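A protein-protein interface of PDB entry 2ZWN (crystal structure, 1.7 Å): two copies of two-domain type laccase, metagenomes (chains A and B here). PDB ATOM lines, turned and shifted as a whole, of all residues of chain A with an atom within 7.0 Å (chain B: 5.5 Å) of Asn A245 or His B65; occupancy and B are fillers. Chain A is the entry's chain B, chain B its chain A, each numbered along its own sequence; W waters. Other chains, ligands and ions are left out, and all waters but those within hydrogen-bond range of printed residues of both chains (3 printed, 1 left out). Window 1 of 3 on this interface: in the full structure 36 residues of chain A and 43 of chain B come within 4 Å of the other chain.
No position is printed for both chains. Of the 9 pairs that touch across the chains among the printed residues, none has its exchanged pair printed and touching as well.
Water W1 bridges the backbone carbonyl oxygen (O) of Val B64 (2.7 Å) and the backbone NH (N) of Gly A207 (2.8 Å). Water W2 lies within hydrogen-bond range of OD1 of Asp A209 (2.8 Å), O of Gly B63 (2.9 Å) and NE2 of His B65 (3.5 Å). Water W3 bridges OD1 of Asn A245 and N of Gly B68.
Among the printed residues, pairs that only touch across the chains: Gly A207 with His B65 (3.3 Å), Asp A244 with Lys B67 (3.3 Å), Asn A245 with Lys B67 (3.4 Å) and Phe A249 with His B65 (3.7 Å).
The backbone NH (N) of Asn A245 lies within hydrogen-bond range of the side-chain hydroxyl (OH) of Tyr A275 (3.1 Å). O of Gly A207 lies within hydrogen-bond range of ND2 of Asn A245. The side-chain amide oxygen (OE1) of Gln B66 sits at hydrogen-bond distance from the side-chain hydroxyl (OG1) of Thr B69, 2.8 Å away. The backbone NH of Asp A244 lies within hydrogen-bond range of the side-chain hydroxyl of Tyr A275 (3.2 Å). The backbone carbonyl oxygen (O) of Phe A249 is in hydrogen-bond range of the backbone NH (N) of Ile A273 (2.7 Å).
Of the 18 printed residues of chain A, 5 touch a printed residue of chain B. Hydrophobic or aromatic side chains of chain A that line the printed part of chain B: Phe A249. Printed residues of chain B that touch a printed residue of chain A: His B65, Gln B66, Lys B67, Gly B68 and Arg B97. Among the printed residues, Asp or Glu carboxylates within 4 Å of a Lys or Arg side-chain nitrogen of the other chain: Asp A209 with Arg B97 (2.9 Å).
His A206 touches none of the printed residues of chain B. Printed residues of chain B within 4 Å of Asp A209: His B65 (2.8 Å) and Arg B97 (2.9 Å). Printed residues of chain B within 4 Å of Asp A244: Lys B67 (3.3 Å). Of chain B, only His B65, Gln B66, Lys B67 and Gly B68 come within 4 Å of Asn A245. His B65 touches four residues of chain A. Printed residues of chain A within 4 Å of Lys B67: Asp A244 and Asn A245. Thr B69 touches none of the printed residues of chain A. The nearest residue of chain A that does not touch His B65 is His A208 (4.3 Å). The nearest printed residue of chain B that does not touch Gly A207 is Val B64 (4.5 Å).
The side-chain carboxylate (OD1) of Asp A209 lies within salt-bridge range of the guanidinium group (NH2) of Arg B97 (2.9 Å). OD2 of Asp A209 is in hydrogen-bond range of NE2 of His B65 (2.8 Å). The side-chain amide oxygen (OD1) of Asn A245 lies close to the backbone carbonyl oxygen (O) of Gln B66 (3.4 Å). The backbone carbonyl oxygen of His B65 sits at hydrogen-bond distance from the side-chain amide nitrogen of Asn A245, at 2.8 Å. N of Gly B68 is in hydrogen-bond range of OD1 of Asn A245 (3.3 Å).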
ATOM      1  N   LYS A 185      34.672  -7.582  14.967  1.00  0.00           N
ATOM      2  CA  LYS A 185      35.015  -8.819  15.648  1.00  0.00           C
ATOM      3  C   LYS A 185      35.594  -8.499  17.024  1.00  0.00           C
ATOM      4  O   LYS A 185      36.486  -7.652  17.148  1.00  0.00           O
ATOM      5  CB  LYS A 185      36.017  -9.640  14.836  1.00  0.00           C
ATOM      6  CG  LYS A 185      36.226 -11.040  15.378  1.00  0.00           C
ATOM      7  CD  LYS A 185      37.171 -11.846  14.520  1.00  0.00           C
ATOM      8  CE  LYS A 185      37.436 -13.207  15.151  1.00  0.00           C
ATOM      9  NZ  LYS A 185      38.513 -13.952  14.444  1.00  0.00           N
ATOM     10  N   GLY A 186      35.082  -9.176  18.048  1.00  0.00           N
ATOM     11  CA  GLY A 186      35.531  -8.956  19.419  1.00  0.00           C
ATOM     12  C   GLY A 186      34.641  -8.029  20.230  1.00  0.00           C
ATOM     13  O   GLY A 186      34.784  -7.951  21.455  1.00  0.00           O
ATOM     14  N   SER A 205      18.290 -13.564  16.482  1.00  0.00           N
ATOM     15  CA  SER A 205      19.597 -13.198  15.950  1.00  0.00           C
ATOM     16  C   SER A 205      20.201 -14.356  15.168  1.00  0.00           C
ATOM     17  O   SER A 205      20.494 -15.407  15.745  1.00  0.00           O
ATOM     18  CB  SER A 205      20.544 -12.816  17.089  1.00  0.00           C
ATOM     19  OG  SER A 205      20.671 -13.862  18.038  1.00  0.00           O
ATOM     20  N   HIS A 206      20.408 -14.165  13.864  1.00  0.00           N
ATOM     21  CA  HIS A 206      21.168 -15.140  13.081  1.00  0.00           C
ATOM     22  C   HIS A 206      22.627 -15.098  13.503  1.00  0.00           C
ATOM     23  O   HIS A 206      23.124 -14.060  13.938  1.00  0.00           O
ATOM     24  CB  HIS A 206      21.094 -14.850  11.582  1.00  0.00           C
ATOM     25  CG  HIS A 206      19.764 -15.136  10.966  1.00  0.00           C
ATOM     26  ND1 HIS A 206      19.642 -15.697   9.713  1.00  0.00           N
ATOM     27  CD2 HIS A 206      18.503 -14.934  11.415  1.00  0.00           C
ATOM     28  CE1 HIS A 206      18.361 -15.827   9.416  1.00  0.00           C
ATOM     29  NE2 HIS A 206      17.648 -15.377  10.434  1.00  0.00           N
ATOM     30  N   GLY A 207      23.297 -16.239  13.386  1.00  0.00           N
ATOM     31  CA  GLY A 207      24.742 -16.323  13.547  1.00  0.00           C
ATOM     32  C   GLY A 207      25.273 -16.281  14.968  1.00  0.00           C
ATOM     33  O   GLY A 207      26.478 -16.436  15.180  1.00  0.00           O
ATOM     34  N   HIS A 208      24.396 -16.057  15.943  1.00  0.00           N
ATOM     35  CA  HIS A 208      24.809 -15.849  17.330  1.00  0.00           C
ATOM     36  C   HIS A 208      23.704 -16.303  18.259  1.00  0.00           C
ATOM     37  O   HIS A 208      22.529 -16.182  17.924  1.00  0.00           O
ATOM     38  CB  HIS A 208      25.047 -14.361  17.634  1.00  0.00           C
ATOM     39  CG  HIS A 208      25.921 -13.655  16.642  1.00  0.00           C
ATOM     40  ND1 HIS A 208      25.472 -13.268  15.395  1.00  0.00           N
ATOM     41  CD2 HIS A 208      27.208 -13.245  16.723  1.00  0.00           C
ATOM     42  CE1 HIS A 208      26.457 -12.675  14.745  1.00  0.00           C
ATOM     43  NE2 HIS A 208      27.519 -12.646  15.529  1.00  0.00           N
ATOM     44  N   ASP A 209      24.096 -16.804  19.426  1.00  0.00           N
ATOM     45  CA  ASP A 209      23.184 -16.922  20.551  1.00  0.00           C
ATOM     46  C   ASP A 209      23.243 -15.654  21.390  1.00  0.00           C
ATOM     47  O   ASP A 209      24.265 -14.962  21.434  1.00  0.00           O
ATOM     48  CB  ASP A 209      23.549 -18.118  21.423  1.00  0.00           C
ATOM     49  CG  ASP A 209      23.274 -19.435  20.740  1.00  0.00           C
ATOM     50  OD1 ASP A 209      22.180 -19.578  20.173  1.00  0.00           O
ATOM     51  OD2 ASP A 209      24.144 -20.328  20.780  1.00  0.00           O
ATOM     52  N   GLU A 242      28.201 -11.889  21.920  1.00  0.00           N
ATOM     53  CA  GLU A 242      29.641 -11.858  21.685  1.00  0.00           C
ATOM     54  C   GLU A 242      29.817 -11.818  20.176  1.00  0.00           C
ATOM     55  O   GLU A 242      29.426 -12.762  19.490  1.00  0.00           O
ATOM     56  CB  GLU A 242      30.310 -13.119  22.234  1.00  0.00           C
ATOM     57  CG  GLU A 242      30.055 -13.406  23.713  1.00  0.00           C
ATOM     58  CD  GLU A 242      30.879 -12.552  24.646  1.00  0.00           C
ATOM     59  OE1 GLU A 242      31.914 -11.998  24.215  1.00  0.00           O
ATOM     60  OE2 GLU A 242      30.495 -12.447  25.830  1.00  0.00           O
ATOM     61  N   ALA A 243      30.405 -10.744  19.660  1.00  0.00           N
ATOM     62  CA  ALA A 243      30.543 -10.577  18.216  1.00  0.00           C
ATOM     63  C   ALA A 243      31.801 -11.303  17.745  1.00  0.00           C
ATOM     64  O   ALA A 243      32.820 -10.677  17.452  1.00  0.00           O
ATOM     65  CB  ALA A 243      30.586  -9.093  17.853  1.00  0.00           C
ATOM     66  N   ASP A 244      31.715 -12.630  17.688  1.00  0.00           N
ATOM     67  CA  ASP A 244      32.875 -13.491  17.424  1.00  0.00           C
ATOM     68  C   ASP A 244      32.762 -14.263  16.108  1.00  0.00           C
ATOM     69  O   ASP A 244      33.516 -15.209  15.874  1.00  0.00           O
ATOM     70  CB  ASP A 244      33.061 -14.478  18.588  1.00  0.00           C
ATOM     71  CG  ASP A 244      31.902 -15.463  18.728  1.00  0.00           C
ATOM     72  OD1 ASP A 244      30.885 -15.342  18.000  1.00  0.00           O
ATOM     73  OD2 ASP A 244      32.008 -16.380  19.583  1.00  0.00           O
ATOM     74  N   ASN A 245      31.836 -13.849  15.247  1.00  0.00           N
ATOM     75  CA  ASN A 245      31.503 -14.611  14.048  1.00  0.00           C
ATOM     76  C   ASN A 245      31.257 -13.678  12.861  1.00  0.00           C
ATOM     77  O   ASN A 245      30.111 -13.409  12.509  1.00  0.00           O
ATOM     78  CB  ASN A 245      30.271 -15.477  14.325  1.00  0.00           C
ATOM     79  CG  ASN A 245      29.918 -16.389  13.162  1.00  0.00           C
ATOM     80  OD1 ASN A 245      30.741 -16.635  12.273  1.00  0.00           O
ATOM     81  ND2 ASN A 245      28.688 -16.899  13.165  1.00  0.00           N
ATOM     82  N   PRO A 246      32.339 -13.160  12.252  1.00  0.00           N
ATOM     83  CA  PRO A 246      32.209 -12.207  11.150  1.00  0.00           C
ATOM     84  C   PRO A 246      31.350 -12.681   9.977  1.00  0.00           C
ATOM     85  O   PRO A 246      31.522 -13.787   9.468  1.00  0.00           O
ATOM     86  CB  PRO A 246      33.660 -11.977  10.712  1.00  0.00           C
ATOM     87  CG  PRO A 246      34.462 -12.280  11.918  1.00  0.00           C
ATOM     88  CD  PRO A 246      33.750 -13.400  12.595  1.00  0.00           C
ATOM     89  N   GLY A 247      30.432 -11.818   9.563  1.00  0.00           N
ATOM     90  CA  GLY A 247      29.554 -12.075   8.429  1.00  0.00           C
ATOM     91  C   GLY A 247      28.524 -10.970   8.354  1.00  0.00           C
ATOM     92  O   GLY A 247      28.685  -9.930   8.998  1.00  0.00           O
ATOM     93  N   ARG A 248      27.479 -11.189   7.561  1.00  0.00           N
ATOM     94  CA  ARG A 248      26.275 -10.360   7.596  1.00  0.00           C
ATOM     95  C   ARG A 248      25.144 -11.240   8.109  1.00  0.00           C
ATOM     96  O   ARG A 248      24.748 -12.193   7.437  1.00  0.00           O
ATOM     97  CB  ARG A 248      25.933  -9.815   6.210  1.00  0.00           C
ATOM     98  CG  ARG A 248      26.982  -8.857   5.653  1.00  0.00           C
ATOM     99  CD  ARG A 248      26.445  -8.080   4.476  1.00  0.00           C
ATOM    100  NE  ARG A 248      26.121  -8.933   3.330  1.00  0.00           N
ATOM    101  CZ  ARG A 248      26.961  -9.248   2.340  1.00  0.00           C
ATOM    102  NH1 ARG A 248      28.215  -8.802   2.322  1.00  0.00           N
ATOM    103  NH2 ARG A 248      26.544 -10.022   1.347  1.00  0.00           N
ATOM    104  N   PHE A 249      24.641 -10.923   9.304  1.00  0.00           N
ATOM    105  CA  PHE A 249      23.673 -11.775   9.990  1.00  0.00           C
ATOM    106  C   PHE A 249      22.397 -11.014  10.335  1.00  0.00           C
ATOM    107  O   PHE A 249      22.402 -10.098  11.155  1.00  0.00           O
ATOM    108  CB  PHE A 249      24.302 -12.376  11.243  1.00  0.00           C
ATOM    109  CG  PHE A 249      25.230 -13.528  10.952  1.00  0.00           C
ATOM    110  CD1 PHE A 249      24.734 -14.712  10.418  1.00  0.00           C
ATOM    111  CD2 PHE A 249      26.590 -13.427  11.195  1.00  0.00           C
ATOM    112  CE1 PHE A 249      25.578 -15.780  10.145  1.00  0.00           C
ATOM    113  CE2 PHE A 249      27.437 -14.491  10.921  1.00  0.00           C
ATOM    114  CZ  PHE A 249      26.930 -15.669  10.400  1.00  0.00           C
ATOM    115  N   ILE A 273      23.224  -7.503  11.531  1.00  0.00           N
ATOM    116  CA  ILE A 273      24.487  -7.402  12.238  1.00  0.00           C
ATOM    117  C   ILE A 273      25.557  -7.460  11.144  1.00  0.00           C
ATOM    118  O   ILE A 273      25.772  -8.512  10.541  1.00  0.00           O
ATOM    119  CB  ILE A 273      24.682  -8.556  13.236  1.00  0.00           C
ATOM    120  CG1 ILE A 273      23.596  -8.533  14.315  1.00  0.00           C
ATOM    121  CG2 ILE A 273      26.053  -8.481  13.891  1.00  0.00           C
ATOM    122  CD1 ILE A 273      23.507  -9.837  15.090  1.00  0.00           C
ATOM    123  N   TYR A 275      29.420  -7.020  10.250  1.00  0.00           N
ATOM    124  CA  TYR A 275      30.770  -6.924  10.784  1.00  0.00           C
ATOM    125  C   TYR A 275      31.652  -6.091   9.867  1.00  0.00           C
ATOM    126  O   TYR A 275      31.579  -6.237   8.646  1.00  0.00           O
ATOM    127  CB  TYR A 275      31.402  -8.300  10.911  1.00  0.00           C
ATOM    128  CG  TYR A 275      30.975  -9.110  12.102  1.00  0.00           C
ATOM    129  CD1 TYR A 275      29.695  -9.656  12.183  1.00  0.00           C
ATOM    130  CD2 TYR A 275      31.879  -9.397  13.124  1.00  0.00           C
ATOM    131  CE1 TYR A 275      29.321 -10.440  13.267  1.00  0.00           C
ATOM    132  CE2 TYR A 275      31.514 -10.177  14.205  1.00  0.00           C
ATOM    133  CZ  TYR A 275      30.239 -10.701  14.269  1.00  0.00           C
ATOM    134  OH  TYR A 275      29.899 -11.478  15.341  1.00  0.00           O
ATOM    135  N   VAL A 278      33.880  -7.335   6.260  1.00  0.00           N
ATOM    136  CA  VAL A 278      33.245  -8.367   5.443  1.00  0.00           C
ATOM    137  C   VAL A 278      32.978  -7.788   4.043  1.00  0.00           C
ATOM    138  O   VAL A 278      32.288  -6.775   3.918  1.00  0.00           O
ATOM    139  CB  VAL A 278      31.926  -8.878   6.077  1.00  0.00           C
ATOM    140  CG1 VAL A 278      31.288  -9.930   5.190  1.00  0.00           C
ATOM    141  CG2 VAL A 278      32.195  -9.449   7.475  1.00  0.00           C
ATOM    142  N   GLY B  63      19.411 -21.628  14.261  1.00  0.00           N
ATOM    143  CA  GLY B  63      20.164 -22.105  15.407  1.00  0.00           C
ATOM    144  C   GLY B  63      21.606 -22.399  15.044  1.00  0.00           C
ATOM    145  O   GLY B  63      22.462 -22.391  15.917  1.00  0.00           O
ATOM    146  N   VAL B  64      21.878 -22.662  13.762  1.00  0.00           N
ATOM    147  CA  VAL B  64      23.235 -22.943  13.311  1.00  0.00           C
ATOM    148  C   VAL B  64      24.002 -21.625  13.252  1.00  0.00           C
ATOM    149  O   VAL B  64      23.559 -20.679  12.609  1.00  0.00           O
ATOM    150  CB  VAL B  64      23.249 -23.652  11.927  1.00  0.00           C
ATOM    151  CG1 VAL B  64      24.676 -23.862  11.425  1.00  0.00           C
ATOM    152  CG2 VAL B  64      22.532 -24.991  12.014  1.00  0.00           C
ATOM    153  N   HIS B  65      25.145 -21.568  13.933  1.00  0.00           N
ATOM    154  CA  HIS B  65      25.925 -20.332  14.023  1.00  0.00           C
ATOM    155  C   HIS B  65      26.517 -19.906  12.690  1.00  0.00           C
ATOM    156  O   HIS B  65      26.703 -18.718  12.455  1.00  0.00           O
ATOM    157  CB  HIS B  65      27.073 -20.473  15.029  1.00  0.00           C
ATOM    158  CG  HIS B  65      26.631 -20.510  16.457  1.00  0.00           C
ATOM    159  ND1 HIS B  65      27.420 -21.019  17.464  1.00  0.00           N
ATOM    160  CD2 HIS B  65      25.477 -20.114  17.044  1.00  0.00           C
ATOM    161  CE1 HIS B  65      26.775 -20.924  18.615  1.00  0.00           C
ATOM    162  NE2 HIS B  65      25.594 -20.376  18.387  1.00  0.00           N
ATOM    163  N   GLN B  66      26.833 -20.882  11.844  1.00  0.00           N
ATOM    164  CA  GLN B  66      27.534 -20.646  10.587  1.00  0.00           C
ATOM    165  C   GLN B  66      28.882 -19.989  10.874  1.00  0.00           C
ATOM    166  O   GLN B  66      29.239 -18.984  10.257  1.00  0.00           O
ATOM    167  CB  GLN B  66      26.696 -19.795   9.621  1.00  0.00           C
ATOM    168  CG  GLN B  66      25.312 -20.355   9.295  1.00  0.00           C
ATOM    169  CD  GLN B  66      25.340 -21.571   8.377  1.00  0.00           C
ATOM    170  OE1 GLN B  66      26.394 -21.969   7.872  1.00  0.00           O
ATOM    171  NE2 GLN B  66      24.165 -22.165   8.147  1.00  0.00           N
ATOM    172  N   LYS B  67      29.620 -20.578  11.817  1.00  0.00           N
ATOM    173  CA  LYS B  67      30.930 -20.074  12.231  1.00  0.00           C
ATOM    174  C   LYS B  67      31.889 -20.141  11.046  1.00  0.00           C
ATOM    175  O   LYS B  67      32.289 -21.227  10.619  1.00  0.00           O
ATOM    176  CB  LYS B  67      31.475 -20.892  13.408  1.00  0.00           C
ATOM    177  CG  LYS B  67      32.633 -20.235  14.152  1.00  0.00           C
ATOM    178  CD  LYS B  67      32.131 -19.339  15.280  1.00  0.00           C
ATOM    179  CE  LYS B  67      33.234 -18.448  15.849  1.00  0.00           C
ATOM    180  NZ  LYS B  67      34.436 -19.216  16.323  1.00  0.00           N
ATOM    181  N   GLY B  68      32.218 -18.976  10.497  1.00  0.00           N
ATOM    182  CA  GLY B  68      33.059 -18.879   9.313  1.00  0.00           C
ATOM    183  C   GLY B  68      32.405 -19.335   8.016  1.00  0.00           C
ATOM    184  O   GLY B  68      33.096 -19.531   7.016  1.00  0.00           O
ATOM    185  N   THR B  69      31.083 -19.501   8.021  1.00  0.00           N
ATOM    186  CA  THR B  69      30.352 -19.998   6.854  1.00  0.00           C
ATOM    187  C   THR B  69      29.054 -19.212   6.648  1.00  0.00           C
ATOM    188  O   THR B  69      28.040 -19.771   6.219  1.00  0.00           O
ATOM    189  CB  THR B  69      30.025 -21.513   6.985  1.00  0.00           C
ATOM    190  OG1 THR B  69      29.168 -21.728   8.114  1.00  0.00           O
ATOM    191  CG2 THR B  69      31.297 -22.337   7.167  1.00  0.00           C
ATOM    192  N   ASP B  96      28.337 -27.239  15.027  1.00  0.00           N
ATOM    193  CA  ASP B  96      28.978 -27.006  16.327  1.00  0.00           C
ATOM    194  C   ASP B  96      28.016 -26.460  17.385  1.00  0.00           C
ATOM    195  O   ASP B  96      28.377 -26.366  18.547  1.00  0.00           O
ATOM    196  CB  ASP B  96      30.239 -26.128  16.213  1.00  0.00           C
ATOM    197  CG  ASP B  96      30.000 -24.792  15.518  1.00  0.00           C
ATOM    198  OD1 ASP B  96      28.843 -24.361  15.356  1.00  0.00           O
ATOM    199  OD2 ASP B  96      31.012 -24.161  15.136  1.00  0.00           O
ATOM    200  N   ARG B  97      26.803 -26.094  16.978  1.00  0.00           N
ATOM    201  CA  ARG B  97      25.761 -25.683  17.922  1.00  0.00           C
ATOM    202  C   ARG B  97      24.853 -26.876  18.183  1.00  0.00           C
ATOM    203  O   ARG B  97      24.267 -27.431  17.260  1.00  0.00           O
ATOM    204  CB  ARG B  97      24.956 -24.510  17.355  1.00  0.00           C
ATOM    205  CG  ARG B  97      23.651 -24.198  18.088  1.00  0.00           C
ATOM    206  CD  ARG B  97      23.852 -23.743  19.508  1.00  0.00           C
ATOM    207  NE  ARG B  97      22.819 -22.768  19.864  1.00  0.00           N
ATOM    208  CZ  ARG B  97      21.550 -23.063  20.143  1.00  0.00           C
ATOM    209  NH1 ARG B  97      21.120 -24.316  20.126  1.00  0.00           N
ATOM    210  NH2 ARG B  97      20.706 -22.083  20.446  1.00  0.00           N
HETATM  211  O   HOH W   1      22.403 -18.387  11.746  1.00  0.00           O
HETATM  212  O   HOH W   2      22.284 -19.922  17.445  1.00  0.00           O
HETATM  213  O   HOH W   3      33.424 -16.722  11.649  1.00  0.00           O
